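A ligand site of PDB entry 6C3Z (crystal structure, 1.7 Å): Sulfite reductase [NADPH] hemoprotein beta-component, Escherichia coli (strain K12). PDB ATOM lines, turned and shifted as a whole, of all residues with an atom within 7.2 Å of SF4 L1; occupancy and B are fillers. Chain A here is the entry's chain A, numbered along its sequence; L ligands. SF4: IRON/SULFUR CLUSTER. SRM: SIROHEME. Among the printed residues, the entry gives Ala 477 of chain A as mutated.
A sulfur (S3) of SF4 L1 sits close to the backbone NH (N) of Ser 436 (3.7 Å).
The side-chain amide nitrogen of Asn 481 lies close to a sulfur (S1) of SF4 L1 (3.6 Å).
The backbone NH (N) of Val 435 is in hydrogen-bond range of an oxygen (O3B) of SRM L2 (3.3 Å).
SG of Cys 434 binds FE1 of SF4 L1 (2.4 Å).
SG of Cys 440 is bound to FE2 of SF4 L1, 2.4 Å away.
The backbone NH (N) of Cys 483 sits close to a sulfur (S2) of SF4 L1.
O4C of SRM L2 lies within salt-bridge range of NH1 of Arg 485.
SG of Cys 479 is bound to FE3 of SF4 L1.
An iron atom (FE) of SRM L2 is bound by the side-chain sulfur (SG) of Cys 483 (2.5 Å).
The side-chain hydroxyl (OG1) of Thr 439 sits at hydrogen-bond distance from an oxygen (O1A) of SRM L2 (2.9 Å).
SG of Cys 483 is bound to FE4 of SF4 L1.
The backbone NH (N) of Cys 479 sits close to a sulfur (S4) of SF4 L1, 3.8 Å away.
Residues that only touch SF4 L1: Gly 478 (3.6 Å), Ala 443 (3.6 Å) and Gly 482 (3.9 Å).
Hydrophobic or aromatic side chains that line SF4 L1: Ala 443.
Of the 23 residues printed, 9 come within 4 Å of SF4 L1.
The nearest printed residue that does not touch SF4 L1 is Leu 442 (4.004 Å).
The backbone NH of Ala 445 is in hydrogen-bond range of the backbone carbonyl oxygen of Gly 478.
The side-chain hydroxyl (OG) of Ser 436 lies within hydrogen-bond range of the backbone carbonyl oxygen (O) of Ala 445.
N of Gly 478 lies close to SG of Cys 434, 3.2 Å away.
SG of Cys 440 sits close to N of Leu 442 (3.3 Å).
The backbone NH (N) of Met 444 is in hydrogen-bond range of the backbone carbonyl oxygen (O) of Gly 478 (2.9 Å).
SG of Cys 479 sits close to N of Asn 481 (3.5 Å).
N of Cys 434 sits at hydrogen-bond distance from O of Val 476.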
ATOM      1  N   ALA A 433       4.085  19.332  24.478  1.00  0.00           N
ATOM      2  CA  ALA A 433       4.295  20.052  23.232  1.00  0.00           C
ATOM      3  C   ALA A 433       3.157  21.063  23.052  1.00  0.00           C
ATOM      4  O   ALA A 433       2.044  20.839  23.511  1.00  0.00           O
ATOM      5  CB  ALA A 433       4.354  19.107  22.031  1.00  0.00           C
ATOM      6  N   CYS A 434       3.446  22.170  22.376  1.00  0.00           N
ATOM      7  CA  CYS A 434       2.408  23.129  22.032  1.00  0.00           C
ATOM      8  C   CYS A 434       1.601  22.656  20.831  1.00  0.00           C
ATOM      9  O   CYS A 434       1.903  21.627  20.203  1.00  0.00           O
ATOM     10  CB  CYS A 434       3.009  24.493  21.725  1.00  0.00           C
ATOM     11  SG  CYS A 434       4.056  24.350  20.256  1.00  0.00           S
ATOM     12  N   VAL A 435       0.587  23.433  20.465  1.00  0.00           N
ATOM     13  CA  VAL A 435      -0.292  23.056  19.353  1.00  0.00           C
ATOM     14  C   VAL A 435       0.472  23.056  18.021  1.00  0.00           C
ATOM     15  O   VAL A 435       0.465  22.058  17.286  1.00  0.00           O
ATOM     16  CB  VAL A 435      -1.514  23.987  19.294  1.00  0.00           C
ATOM     17  CG1 VAL A 435      -2.316  23.736  18.026  1.00  0.00           C
ATOM     18  CG2 VAL A 435      -2.376  23.765  20.526  1.00  0.00           C
ATOM     19  N   SER A 436       1.114  24.167  17.688  1.00  0.00           N
ATOM     20  CA  SER A 436       1.922  24.315  16.434  1.00  0.00           C
ATOM     21  C   SER A 436       1.064  23.974  15.205  1.00  0.00           C
ATOM     22  O   SER A 436      -0.144  24.279  15.184  1.00  0.00           O
ATOM     23  CB  SER A 436       3.187  23.477  16.561  1.00  0.00           C
ATOM     24  OG  SER A 436       3.968  23.575  15.353  1.00  0.00           O
ATOM     25  N   PHE A 437       1.642  23.369  14.162  1.00  0.00           N
ATOM     26  CA  PHE A 437       0.877  22.957  12.985  1.00  0.00           C
ATOM     27  C   PHE A 437      -0.181  21.911  13.384  1.00  0.00           C
ATOM     28  O   PHE A 437       0.041  21.112  14.306  1.00  0.00           O
ATOM     29  CB  PHE A 437       1.792  22.366  11.903  1.00  0.00           C
ATOM     30  CG  PHE A 437       2.850  23.306  11.390  1.00  0.00           C
ATOM     31  CD1 PHE A 437       2.501  24.415  10.628  1.00  0.00           C
ATOM     32  CD2 PHE A 437       4.198  23.042  11.614  1.00  0.00           C
ATOM     33  CE1 PHE A 437       3.478  25.274  10.128  1.00  0.00           C
ATOM     34  CE2 PHE A 437       5.185  23.898  11.116  1.00  0.00           C
ATOM     35  CZ  PHE A 437       4.825  25.024  10.385  1.00  0.00           C
ATOM     36  N   THR A 439      -2.693  24.270  12.834  1.00  0.00           N
ATOM     37  CA  THR A 439      -3.539  25.435  13.074  1.00  0.00           C
ATOM     38  C   THR A 439      -2.773  26.703  13.469  1.00  0.00           C
ATOM     39  O   THR A 439      -3.300  27.801  13.243  1.00  0.00           O
ATOM     40  CB  THR A 439      -4.561  25.122  14.185  1.00  0.00           C
ATOM     41  OG1 THR A 439      -3.878  24.571  15.326  1.00  0.00           O
ATOM     42  CG2 THR A 439      -5.604  24.138  13.690  1.00  0.00           C
ATOM     43  N   CYS A 440      -1.573  26.597  14.017  1.00  0.00           N
ATOM     44  CA  CYS A 440      -0.919  27.819  14.489  1.00  0.00           C
ATOM     45  C   CYS A 440      -0.298  28.575  13.320  1.00  0.00           C
ATOM     46  O   CYS A 440       0.541  28.021  12.603  1.00  0.00           O
ATOM     47  CB  CYS A 440       0.160  27.544  15.490  1.00  0.00           C
ATOM     48  SG  CYS A 440       0.824  29.097  16.060  1.00  0.00           S
ATOM     49  N   PRO A 441      -0.607  29.856  13.154  1.00  0.00           N
ATOM     50  CA  PRO A 441      -0.014  30.598  12.030  1.00  0.00           C
ATOM     51  C   PRO A 441       1.433  30.991  12.275  1.00  0.00           C
ATOM     52  O   PRO A 441       2.084  31.493  11.343  1.00  0.00           O
ATOM     53  CB  PRO A 441      -0.939  31.825  11.915  1.00  0.00           C
ATOM     54  CG  PRO A 441      -1.424  32.053  13.314  1.00  0.00           C
ATOM     55  CD  PRO A 441      -1.480  30.696  13.991  1.00  0.00           C
ATOM     56  N   LEU A 442       1.970  30.794  13.477  1.00  0.00           N
ATOM     57  CA  LEU A 442       3.313  31.253  13.772  1.00  0.00           C
ATOM     58  C   LEU A 442       4.320  30.120  13.798  1.00  0.00           C
ATOM     59  O   LEU A 442       5.509  30.357  14.025  1.00  0.00           O
ATOM     60  CB  LEU A 442       3.331  32.006  15.104  1.00  0.00           C
ATOM     61  CG  LEU A 442       2.219  33.041  15.268  1.00  0.00           C
ATOM     62  CD1 LEU A 442       2.337  33.733  16.599  1.00  0.00           C
ATOM     63  CD2 LEU A 442       2.302  34.026  14.106  1.00  0.00           C
ATOM     64  N   ALA A 443       3.858  28.907  13.548  1.00  0.00           N
ATOM     65  CA  ALA A 443       4.672  27.738  13.839  1.00  0.00           C
ATOM     66  C   ALA A 443       5.819  27.645  12.845  1.00  0.00           C
ATOM     67  O   ALA A 443       5.686  28.009  11.667  1.00  0.00           O
ATOM     68  CB  ALA A 443       3.811  26.470  13.815  1.00  0.00           C
ATOM     69  N   MET A 444       6.957  27.177  13.336  1.00  0.00           N
ATOM     70  CA  MET A 444       8.145  26.940  12.516  1.00  0.00           C
ATOM     71  C   MET A 444       8.441  25.462  12.343  1.00  0.00           C
ATOM     72  O   MET A 444       8.849  25.044  11.252  1.00  0.00           O
ATOM     73  CB  MET A 444       9.348  27.647  13.145  1.00  0.00           C
ATOM     74  CG  MET A 444       9.126  29.147  13.435  1.00  0.00           C
ATOM     75  SD  MET A 444      10.591  30.012  14.058  1.00  0.00           S
ATOM     76  CE  MET A 444      10.036  31.715  14.053  1.00  0.00           C
ATOM     77  N   ALA A 445       8.245  24.649  13.378  1.00  0.00           N
ATOM     78  CA  ALA A 445       8.429  23.213  13.274  1.00  0.00           C
ATOM     79  C   ALA A 445       7.261  22.535  13.980  1.00  0.00           C
ATOM     80  O   ALA A 445       6.575  23.141  14.805  1.00  0.00           O
ATOM     81  CB  ALA A 445       9.774  22.766  13.890  1.00  0.00           C
ATOM     82  N   ALA A 447       5.094  20.428  16.511  1.00  0.00           N
ATOM     83  CA  ALA A 447       5.293  20.166  17.924  1.00  0.00           C
ATOM     84  C   ALA A 447       4.342  19.080  18.398  1.00  0.00           C
ATOM     85  O   ALA A 447       4.778  17.960  18.659  1.00  0.00           O
ATOM     86  CB  ALA A 447       5.126  21.448  18.742  1.00  0.00           C
ATOM     87  N   VAL A 476       8.525  20.489  23.819  1.00  0.00           N
ATOM     88  CA  VAL A 476       8.750  20.979  22.461  1.00  0.00           C
ATOM     89  C   VAL A 476       7.893  22.215  22.225  1.00  0.00           C
ATOM     90  O   VAL A 476       6.676  22.175  22.422  1.00  0.00           O
ATOM     91  CB  VAL A 476       8.426  19.882  21.429  1.00  0.00           C
ATOM     92  CG1 VAL A 476       8.743  20.338  20.012  1.00  0.00           C
ATOM     93  CG2 VAL A 476       9.187  18.595  21.766  1.00  0.00           C
ATOM     94  N   ALA A 477       8.514  23.315  21.784  1.00  0.00           N
ATOM     95  CA  ALA A 477       7.784  24.456  21.258  1.00  0.00           C
ATOM     96  C   ALA A 477       7.989  24.541  19.753  1.00  0.00           C
ATOM     97  O   ALA A 477       9.109  24.355  19.259  1.00  0.00           O
ATOM     98  CB  ALA A 477       8.218  25.770  21.933  1.00  0.00           C
ATOM     99  N   GLY A 478       6.919  24.812  19.015  1.00  0.00           N
ATOM    100  CA  GLY A 478       7.010  24.922  17.569  1.00  0.00           C
ATOM    101  C   GLY A 478       7.656  26.194  17.060  1.00  0.00           C
ATOM    102  O   GLY A 478       7.966  26.271  15.877  1.00  0.00           O
ATOM    103  N   CYS A 479       7.854  27.189  17.925  1.00  0.00           N
ATOM    104  CA  CYS A 479       8.570  28.408  17.594  1.00  0.00           C
ATOM    105  C   CYS A 479       8.999  29.051  18.913  1.00  0.00           C
ATOM    106  O   CYS A 479       8.685  28.520  19.984  1.00  0.00           O
ATOM    107  CB  CYS A 479       7.688  29.338  16.743  1.00  0.00           C
ATOM    108  SG  CYS A 479       6.717  30.437  17.667  1.00  0.00           S
ATOM    109  N   PRO A 480       9.781  30.129  18.895  1.00  0.00           N
ATOM    110  CA  PRO A 480      10.330  30.634  20.160  1.00  0.00           C
ATOM    111  C   PRO A 480       9.393  31.503  20.986  1.00  0.00           C
ATOM    112  O   PRO A 480       9.807  31.990  22.050  1.00  0.00           O
ATOM    113  CB  PRO A 480      11.564  31.417  19.703  1.00  0.00           C
ATOM    114  CG  PRO A 480      11.220  31.900  18.352  1.00  0.00           C
ATOM    115  CD  PRO A 480      10.428  30.768  17.734  1.00  0.00           C
ATOM    116  N   ASN A 481       8.137  31.711  20.571  1.00  0.00           N
ATOM    117  CA  ASN A 481       7.168  32.296  21.490  1.00  0.00           C
ATOM    118  C   ASN A 481       7.090  31.502  22.784  1.00  0.00           C
ATOM    119  O   ASN A 481       6.830  32.066  23.857  1.00  0.00           O
ATOM    120  CB  ASN A 481       5.788  32.369  20.829  1.00  0.00           C
ATOM    121  CG  ASN A 481       5.708  33.481  19.800  1.00  0.00           C
ATOM    122  OD1 ASN A 481       6.391  34.511  19.932  1.00  0.00           O
ATOM    123  ND2 ASN A 481       4.902  33.276  18.739  1.00  0.00           N
ATOM    124  N   GLY A 482       7.308  30.190  22.704  1.00  0.00           N
ATOM    125  CA  GLY A 482       7.541  29.383  23.876  1.00  0.00           C
ATOM    126  C   GLY A 482       6.324  28.778  24.518  1.00  0.00           C
ATOM    127  O   GLY A 482       6.380  28.396  25.702  1.00  0.00           O
ATOM    128  N   CYS A 483       5.211  28.666  23.786  1.00  0.00           N
ATOM    129  CA  CYS A 483       3.982  28.177  24.401  1.00  0.00           C
ATOM    130  C   CYS A 483       4.158  26.808  25.008  1.00  0.00           C
ATOM    131  O   CYS A 483       3.519  26.497  26.014  1.00  0.00           O
ATOM    132  CB  CYS A 483       2.871  28.146  23.359  1.00  0.00           C
ATOM    133  SG  CYS A 483       2.734  29.758  22.610  1.00  0.00           S
ATOM    134  N   GLY A 484       5.033  25.982  24.445  1.00  0.00           N
ATOM    135  CA  GLY A 484       5.236  24.690  25.058  1.00  0.00           C
ATOM    136  C   GLY A 484       5.999  24.737  26.371  1.00  0.00           C
ATOM    137  O   GLY A 484       6.150  23.680  26.984  1.00  0.00           O
ATOM    138  N   ARG A 485       6.495  25.911  26.785  1.00  0.00           N
ATOM    139  CA  ARG A 485       7.292  26.063  28.003  1.00  0.00           C
ATOM    140  C   ARG A 485       8.574  25.245  27.930  1.00  0.00           C
ATOM    141  O   ARG A 485       9.039  24.715  28.957  1.00  0.00           O
ATOM    142  CB  ARG A 485       6.482  25.714  29.253  1.00  0.00           C
ATOM    143  CG  ARG A 485       5.264  26.613  29.355  1.00  0.00           C
ATOM    144  CD  ARG A 485       4.812  26.786  30.812  1.00  0.00           C
ATOM    145  NE  ARG A 485       4.309  25.561  31.422  1.00  0.00           N
ATOM    146  CZ  ARG A 485       3.023  25.213  31.461  1.00  0.00           C
ATOM    147  NH1 ARG A 485       2.128  26.010  30.910  1.00  0.00           N
ATOM    148  NH2 ARG A 485       2.630  24.105  32.050  1.00  0.00           N
HETATM  149 FE1  SF4 L   1       3.851  26.574  19.375  1.00  0.00          FE
HETATM  150 FE2  SF4 L   1       2.272  28.355  17.792  1.00  0.00          FE
HETATM  151 FE3  SF4 L   1       4.907  29.020  18.430  1.00  0.00          FE
HETATM  152 FE4  SF4 L   1       2.925  28.951  20.446  1.00  0.00          FE
HETATM  153  S1  SF4 L   1       3.081  30.167  18.652  1.00  0.00           S
HETATM  154  S2  SF4 L   1       4.962  28.112  20.406  1.00  0.00           S
HETATM  155  S3  SF4 L   1       1.815  27.254  19.641  1.00  0.00           S
HETATM  156  S4  SF4 L   1       4.117  27.309  17.336  1.00  0.00           S
HETATM  157 FE   SRM L   2       0.588  30.855  23.441  1.00  0.00          FE
HETATM  158  CHA SRM L   2       0.488  32.866  20.739  1.00  0.00           C
HETATM  159  CHB SRM L   2      -1.130  28.476  21.728  1.00  0.00           C
HETATM  160  CHC SRM L   2       0.423  28.948  26.225  1.00  0.00           C
HETATM  161  CHD SRM L   2       3.142  32.633  24.731  1.00  0.00           C
HETATM  162  NA  SRM L   2      -0.222  30.746  21.623  1.00  0.00           N
HETATM  163  C1A SRM L   2      -0.239  31.709  20.662  1.00  0.00           C
HETATM  164  C2A SRM L   2      -1.203  31.410  19.540  1.00  0.00           C
HETATM  165  CMA SRM L   2      -2.553  32.073  19.812  1.00  0.00           C
HETATM  166  CDA SRM L   2      -0.592  31.777  18.178  1.00  0.00           C
HETATM  167  CEA SRM L   2      -1.093  33.074  17.566  1.00  0.00           C
HETATM  168  O3A SRM L   2      -0.802  34.195  18.051  1.00  0.00           O
HETATM  169  O4A SRM L   2      -1.781  33.037  16.517  1.00  0.00           O
HETATM  170  C3A SRM L   2      -1.305  29.935  19.688  1.00  0.00           C
HETATM  171  CAA SRM L   2      -2.541  29.352  19.044  1.00  0.00           C
HETATM  172  CBA SRM L   2      -2.166  28.007  18.444  1.00  0.00           C
HETATM  173  CCA SRM L   2      -3.413  27.215  18.124  1.00  0.00           C
HETATM  174  O1A SRM L   2      -3.756  26.989  16.939  1.00  0.00           O
HETATM  175  O2A SRM L   2      -4.126  26.755  19.042  1.00  0.00           O
HETATM  176  C4A SRM L   2      -0.844  29.669  21.069  1.00  0.00           C
HETATM  177  NB  SRM L   2      -0.327  29.178  23.910  1.00  0.00           N
HETATM  178  C1B SRM L   2      -0.912  28.272  23.086  1.00  0.00           C
HETATM  179  C2B SRM L   2      -1.300  27.034  23.836  1.00  0.00           C
HETATM  180  CMB SRM L   2      -2.635  26.528  23.298  1.00  0.00           C
HETATM  181  CDB SRM L   2      -0.218  25.961  23.773  1.00  0.00           C
HETATM  182  CEB SRM L   2      -0.637  24.585  24.263  1.00  0.00           C
HETATM  183  O3B SRM L   2      -0.314  23.581  23.594  1.00  0.00           O
HETATM  184  O4B SRM L   2      -1.289  24.386  25.321  1.00  0.00           O
HETATM  185  C3B SRM L   2      -1.454  27.596  25.223  1.00  0.00           C
HETATM  186  CAB SRM L   2      -2.876  28.095  25.449  1.00  0.00           C
HETATM  187  CBB SRM L   2      -2.945  28.721  26.848  1.00  0.00           C
HETATM  188  CCB SRM L   2      -4.222  29.487  27.130  1.00  0.00           C
HETATM  189  O1B SRM L   2      -5.290  28.856  27.243  1.00  0.00           O
HETATM  190  O2B SRM L   2      -4.286  30.741  27.284  1.00  0.00           O
HETATM  191  C4B SRM L   2      -0.380  28.614  25.159  1.00  0.00           C
HETATM  192  NC  SRM L   2       1.621  30.773  25.115  1.00  0.00           N
HETATM  193  C1C SRM L   2       1.416  29.916  26.146  1.00  0.00           C
HETATM  194  C2C SRM L   2       2.431  30.096  27.219  1.00  0.00           C
HETATM  195  CDC SRM L   2       2.714  29.084  28.289  1.00  0.00           C
HETATM  196  CEC SRM L   2       1.913  29.544  29.474  1.00  0.00           C
HETATM  197  O3C SRM L   2       1.263  30.609  29.437  1.00  0.00           O
HETATM  198  O4C SRM L   2       1.885  28.850  30.529  1.00  0.00           O
HETATM  199  C3C SRM L   2       3.392  31.046  26.676  1.00  0.00           C
HETATM  200  CAC SRM L   2       4.821  31.252  27.173  1.00  0.00           C
HETATM  201  CBC SRM L   2       4.952  32.043  28.496  1.00  0.00           C
HETATM  202  CCC SRM L   2       4.964  33.530  28.165  1.00  0.00           C
HETATM  203  O1C SRM L   2       3.906  34.104  27.808  1.00  0.00           O
HETATM  204  O2C SRM L   2       6.022  34.219  28.242  1.00  0.00           O
HETATM  205  C4C SRM L   2       2.706  31.530  25.433  1.00  0.00           C
HETATM  206  ND  SRM L   2       1.506  32.518  22.918  1.00  0.00           N
HETATM  207  C1D SRM L   2       2.533  33.142  23.583  1.00  0.00           C
HETATM  208  C2D SRM L   2       3.202  34.203  22.746  1.00  0.00           C
HETATM  209  CAD SRM L   2       4.446  35.013  23.040  1.00  0.00           C
HETATM  210  CBD SRM L   2       4.069  36.087  24.038  1.00  0.00           C
HETATM  211  CCD SRM L   2       5.176  37.076  24.252  1.00  0.00           C
HETATM  212  O1D SRM L   2       5.348  37.581  25.397  1.00  0.00           O
HETATM  213  O2D SRM L   2       5.945  37.408  23.316  1.00  0.00           O
HETATM  214  C3D SRM L   2       2.393  34.232  21.529  1.00  0.00           C
HETATM  215  CDD SRM L   2       2.575  35.120  20.308  1.00  0.00           C
HETATM  216  CED SRM L   2       2.102  36.526  20.632  1.00  0.00           C
HETATM  217  O3D SRM L   2       1.451  36.746  21.673  1.00  0.00           O
HETATM  218  O4D SRM L   2       2.352  37.495  19.863  1.00  0.00           O
HETATM  219  C4D SRM L   2       1.386  33.166  21.725  1.00  0.00           C
